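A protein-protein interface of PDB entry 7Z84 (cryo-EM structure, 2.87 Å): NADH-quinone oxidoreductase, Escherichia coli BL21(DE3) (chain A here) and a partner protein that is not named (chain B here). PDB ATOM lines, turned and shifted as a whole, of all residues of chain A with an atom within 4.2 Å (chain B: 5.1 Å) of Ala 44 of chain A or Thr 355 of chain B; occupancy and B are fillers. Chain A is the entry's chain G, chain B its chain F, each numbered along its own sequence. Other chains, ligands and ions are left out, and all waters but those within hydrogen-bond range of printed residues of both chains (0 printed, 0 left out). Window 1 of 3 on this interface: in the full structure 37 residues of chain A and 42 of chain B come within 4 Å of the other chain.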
ATOM      1  N   CYS A  34     -25.248  19.920 -14.121  1.00  0.00           N
ATOM      2  CA  CYS A  34     -24.682  19.715 -12.795  1.00  0.00           C
ATOM      3  C   CYS A  34     -24.979  20.842 -11.818  1.00  0.00           C
ATOM      4  O   CYS A  34     -24.611  20.727 -10.645  1.00  0.00           O
ATOM      5  CB  CYS A  34     -23.167  19.528 -12.890  1.00  0.00           C
ATOM      6  SG  CYS A  34     -22.260  21.042 -13.221  1.00  0.00           S
ATOM      7  N   VAL A  42     -20.807  23.731  -9.451  1.00  0.00           N
ATOM      8  CA  VAL A  42     -19.564  22.968  -9.381  1.00  0.00           C
ATOM      9  C   VAL A  42     -18.792  22.954 -10.687  1.00  0.00           C
ATOM     10  O   VAL A  42     -17.581  22.673 -10.673  1.00  0.00           O
ATOM     11  CB  VAL A  42     -19.834  21.522  -8.912  1.00  0.00           C
ATOM     12  CG1 VAL A  42     -20.047  21.485  -7.413  1.00  0.00           C
ATOM     13  CG2 VAL A  42     -21.021  20.940  -9.649  1.00  0.00           C
ATOM     14  N   GLY A  43     -19.410  23.258 -11.823  1.00  0.00           N
ATOM     15  CA  GLY A  43     -18.714  23.228 -13.095  1.00  0.00           C
ATOM     16  C   GLY A  43     -18.327  21.843 -13.565  1.00  0.00           C
ATOM     17  O   GLY A  43     -17.222  21.657 -14.086  1.00  0.00           O
ATOM     18  N   ALA A  44     -19.212  20.864 -13.397  1.00  0.00           N
ATOM     19  CA  ALA A  44     -18.889  19.482 -13.737  1.00  0.00           C
ATOM     20  C   ALA A  44     -19.311  19.126 -15.160  1.00  0.00           C
ATOM     21  O   ALA A  44     -18.470  18.775 -15.987  1.00  0.00           O
ATOM     22  CB  ALA A  44     -19.542  18.532 -12.728  1.00  0.00           C
ATOM     23  N   CYS A  45     -20.604  19.237 -15.469  1.00  0.00           N
ATOM     24  CA  CYS A  45     -21.121  18.714 -16.731  1.00  0.00           C
ATOM     25  C   CYS A  45     -20.624  19.477 -17.954  1.00  0.00           C
ATOM     26  O   CYS A  45     -20.736  18.959 -19.069  1.00  0.00           O
ATOM     27  CB  CYS A  45     -22.645  18.730 -16.713  1.00  0.00           C
ATOM     28  SG  CYS A  45     -23.328  20.388 -16.687  1.00  0.00           S
ATOM     29  N   ARG A  46     -20.096  20.689 -17.764  1.00  0.00           N
ATOM     30  CA  ARG A  46     -19.575  21.545 -18.837  1.00  0.00           C
ATOM     31  C   ARG A  46     -20.610  21.813 -19.929  1.00  0.00           C
ATOM     32  O   ARG A  46     -20.279  21.929 -21.108  1.00  0.00           O
ATOM     33  CB  ARG A  46     -18.272  21.000 -19.423  1.00  0.00           C
ATOM     34  CG  ARG A  46     -17.232  20.631 -18.374  1.00  0.00           C
ATOM     35  CD  ARG A  46     -16.978  21.763 -17.393  1.00  0.00           C
ATOM     36  NE  ARG A  46     -16.067  22.763 -17.932  1.00  0.00           N
ATOM     37  CZ  ARG A  46     -15.553  23.762 -17.229  1.00  0.00           C
ATOM     38  NH1 ARG A  46     -15.820  23.912 -15.943  1.00  0.00           N
ATOM     39  NH2 ARG A  46     -14.750  24.632 -17.832  1.00  0.00           N
ATOM     40  N   VAL A  91     -21.115  18.583 -26.112  1.00  0.00           N
ATOM     41  CA  VAL A  91     -21.237  18.043 -24.760  1.00  0.00           C
ATOM     42  C   VAL A  91     -22.423  17.088 -24.667  1.00  0.00           C
ATOM     43  O   VAL A  91     -22.320  16.005 -24.070  1.00  0.00           O
ATOM     44  CB  VAL A  91     -21.331  19.190 -23.737  1.00  0.00           C
ATOM     45  CG1 VAL A  91     -21.754  18.676 -22.373  1.00  0.00           C
ATOM     46  CG2 VAL A  91     -19.992  19.890 -23.625  1.00  0.00           C
ATOM     47  N   LEU A  95     -22.201  13.057 -23.906  1.00  0.00           N
ATOM     48  CA  LEU A  95     -23.067  12.380 -22.946  1.00  0.00           C
ATOM     49  C   LEU A  95     -23.896  11.290 -23.609  1.00  0.00           C
ATOM     50  O   LEU A  95     -24.281  10.319 -22.949  1.00  0.00           O
ATOM     51  CB  LEU A  95     -23.983  13.389 -22.257  1.00  0.00           C
ATOM     52  CG  LEU A  95     -23.313  14.319 -21.250  1.00  0.00           C
ATOM     53  CD1 LEU A  95     -24.344  15.210 -20.594  1.00  0.00           C
ATOM     54  CD2 LEU A  95     -22.559  13.511 -20.214  1.00  0.00           C
ATOM     55  N   TRP B 353     -14.435  13.739 -13.483  1.00  0.00           N
ATOM     56  CA  TRP B 353     -15.261  14.828 -12.976  1.00  0.00           C
ATOM     57  C   TRP B 353     -16.059  15.483 -14.094  1.00  0.00           C
ATOM     58  O   TRP B 353     -17.291  15.560 -14.026  1.00  0.00           O
ATOM     59  CB  TRP B 353     -14.391  15.863 -12.264  1.00  0.00           C
ATOM     60  CG  TRP B 353     -15.116  17.087 -11.824  1.00  0.00           C
ATOM     61  CD1 TRP B 353     -14.998  18.338 -12.344  1.00  0.00           C
ATOM     62  CD2 TRP B 353     -16.061  17.186 -10.755  1.00  0.00           C
ATOM     63  NE1 TRP B 353     -15.819  19.210 -11.676  1.00  0.00           N
ATOM     64  CE2 TRP B 353     -16.481  18.525 -10.692  1.00  0.00           C
ATOM     65  CE3 TRP B 353     -16.598  16.268  -9.848  1.00  0.00           C
ATOM     66  CZ2 TRP B 353     -17.411  18.972  -9.760  1.00  0.00           C
ATOM     67  CZ3 TRP B 353     -17.520  16.713  -8.924  1.00  0.00           C
ATOM     68  CH2 TRP B 353     -17.918  18.052  -8.887  1.00  0.00           C
ATOM     69  N   CYS B 354     -15.383  15.948 -15.138  1.00  0.00           N
ATOM     70  CA  CYS B 354     -16.030  16.793 -16.126  1.00  0.00           C
ATOM     71  C   CYS B 354     -16.169  16.081 -17.466  1.00  0.00           C
ATOM     72  O   CYS B 354     -15.351  15.235 -17.835  1.00  0.00           O
ATOM     73  CB  CYS B 354     -15.293  18.135 -16.272  1.00  0.00           C
ATOM     74  SG  CYS B 354     -13.806  18.171 -17.255  1.00  0.00           S
ATOM     75  N   THR B 355     -17.241  16.445 -18.176  1.00  0.00           N
ATOM     76  CA  THR B 355     -17.716  15.688 -19.336  1.00  0.00           C
ATOM     77  C   THR B 355     -16.747  15.598 -20.516  1.00  0.00           C
ATOM     78  O   THR B 355     -16.576  14.482 -21.033  1.00  0.00           O
ATOM     79  CB  THR B 355     -19.072  16.254 -19.779  1.00  0.00           C
ATOM     80  OG1 THR B 355     -20.025  16.101 -18.722  1.00  0.00           O
ATOM     81  CG2 THR B 355     -19.591  15.550 -21.024  1.00  0.00           C
ATOM     82  N   PRO B 356     -16.120  16.686 -21.020  1.00  0.00           N
ATOM     83  CA  PRO B 356     -15.374  16.549 -22.291  1.00  0.00           C
ATOM     84  C   PRO B 356     -14.197  15.594 -22.229  1.00  0.00           C
ATOM     85  O   PRO B 356     -14.068  14.742 -23.109  1.00  0.00           O
ATOM     86  CB  PRO B 356     -14.921  17.986 -22.581  1.00  0.00           C
ATOM     87  CG  PRO B 356     -15.865  18.827 -21.858  1.00  0.00           C
ATOM     88  CD  PRO B 356     -16.090  18.094 -20.588  1.00  0.00           C
ATOM     89  N   CYS B 357     -13.369  15.674 -21.189  1.00  0.00           N
ATOM     90  CA  CYS B 357     -12.276  14.720 -21.019  1.00  0.00           C
ATOM     91  C   CYS B 357     -12.807  13.301 -20.845  1.00  0.00           C
ATOM     92  O   CYS B 357     -12.497  12.414 -21.652  1.00  0.00           O
ATOM     93  CB  CYS B 357     -11.429  15.165 -19.828  1.00  0.00           C
ATOM     94  SG  CYS B 357     -10.259  14.054 -19.004  1.00  0.00           S
ATOM     95  N   ARG B 358     -13.725  13.119 -19.886  1.00  0.00           N
ATOM     96  CA  ARG B 358     -14.209  11.798 -19.487  1.00  0.00           C
ATOM     97  C   ARG B 358     -14.922  11.076 -20.627  1.00  0.00           C
ATOM     98  O   ARG B 358     -14.791   9.855 -20.775  1.00  0.00           O
ATOM     99  CB  ARG B 358     -15.137  11.950 -18.277  1.00  0.00           C
ATOM    100  CG  ARG B 358     -16.213  10.884 -18.128  1.00  0.00           C
ATOM    101  CD  ARG B 358     -17.212  11.230 -17.039  1.00  0.00           C
ATOM    102  NE  ARG B 358     -18.390  11.888 -17.591  1.00  0.00           N
ATOM    103  CZ  ARG B 358     -18.872  13.048 -17.169  1.00  0.00           C
ATOM    104  NH1 ARG B 358     -18.315  13.705 -16.167  1.00  0.00           N
ATOM    105  NH2 ARG B 358     -19.946  13.558 -17.765  1.00  0.00           N
ATOM    106  N   ASP B 359     -15.664  11.808 -21.453  1.00  0.00           N
ATOM    107  CA  ASP B 359     -16.475  11.212 -22.503  1.00  0.00           C
ATOM    108  C   ASP B 359     -15.973  11.498 -23.912  1.00  0.00           C
ATOM    109  O   ASP B 359     -16.621  11.081 -24.874  1.00  0.00           O
ATOM    110  CB  ASP B 359     -17.927  11.681 -22.375  1.00  0.00           C
ATOM    111  CG  ASP B 359     -18.659  11.004 -21.236  1.00  0.00           C
ATOM    112  OD1 ASP B 359     -18.313   9.851 -20.903  1.00  0.00           O
ATOM    113  OD2 ASP B 359     -19.582  11.626 -20.672  1.00  0.00           O
ATOM    114  N   GLY B 360     -14.843  12.186 -24.071  1.00  0.00           N
ATOM    115  CA  GLY B 360     -14.326  12.439 -25.393  1.00  0.00           C
ATOM    116  C   GLY B 360     -12.956  11.843 -25.603  1.00  0.00           C
ATOM    117  O   GLY B 360     -12.588  11.544 -26.743  1.00  0.00           O
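The backbone carbonyl oxygen (O) of Ala 44 of chain A lies within hydrogen-bond range of the backbone NH (N) of Thr 355 of chain B (3.4 Å). OG1 of Thr 355 of chain B lies within hydrogen-bond range of O of Cys 45 of chain A (3.0 Å).
Val 42 of chain A touches Trp 353 of chain B (CB to CZ2, 3.6 Å). NE1 of Trp 353 of chain B touches O of Gly 43 of chain A (3.7 Å). Trp 353 of chain B touches Ala 44 of chain A. Cys 354 of chain B touches Ala 44 of chain A (CA to O, 3.1 Å). Arg 46 of chain A touches Cys 354 of chain B. Arg 46 of chain A touches Pro 356 of chain B. Thr 355 of chain B touches Leu 95 of chain A. CD2 of Leu 95 of chain A touches NH2 of Arg 358 of chain B (3.6 Å). Leu 95 of chain A touches Asp 359 of chain B (CD2 to OD2, 3.6 Å).
Printed residues of chain B within 4 Å of Val 42 of chain A: Trp 353 (3.6 Å). Of the printed residues of chain A, Trp 353 of chain B touches Val 42, Gly 43 and Ala 44. Of chain A, only Ala 44 (3.4 Å), Cys 45 (3.0 Å) and Leu 95 (3.7 Å) come within 4 Å of Thr 355 of chain B. Of the printed residues of chain A, Asp 359 of chain B touches Leu 95. The nearest printed residue of chain B that does not touch Ala 44 of chain A is Arg 358 of chain B (5.1 Å). The nearest residue of chain A that does not touch Thr 355 of chain B is Val 91 of chain A (4.03 Å). The nearest printed residue of chain B that does not touch Cys 45 of chain A is Pro 356 of chain B (5.0 Å).
Hydrophobic or aromatic side chains of chain A within 4 Å of the printed part of chain B: Val 42, Ala 44 and Leu 95. Printed residues of chain B that touch a printed residue of chain A: Trp 353, Cys 354, Thr 355, Pro 356, Arg 358 and Asp 359. Hydrophobic or aromatic side chains of chain B within 4 Å of the printed part of chain A: Trp 353 and Pro 356. Along chain B the printed residues that touch a printed residue of chain A span positions 353 to 359. Among the printed residues, no Asp or Glu carboxylate lies within 4 Å of a Lys or Arg side-chain nitrogen of the other chain.
The backbone carbonyl oxygen of Trp 353 of chain B lies within hydrogen-bond range of the guanidinium group of Arg 358 of chain B. The guanidinium group of Arg 358 of chain B is in hydrogen-bond range of the side-chain hydroxyl of Thr 355 of chain B (2.7 Å). The guanidinium group of Arg 358 of chain B is in salt-bridge range of the side-chain carboxylate of Asp 359 of chain B (3.3 Å). The side-chain sulfur of Cys 34 of chain A lies close to the backbone NH of Ala 44 of chain A. The guanidinium group (NH1) of Arg 46 of chain A sits at hydrogen-bond distance from the backbone carbonyl oxygen (O) of Gly 43 of chain A, 3.2 Å away.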
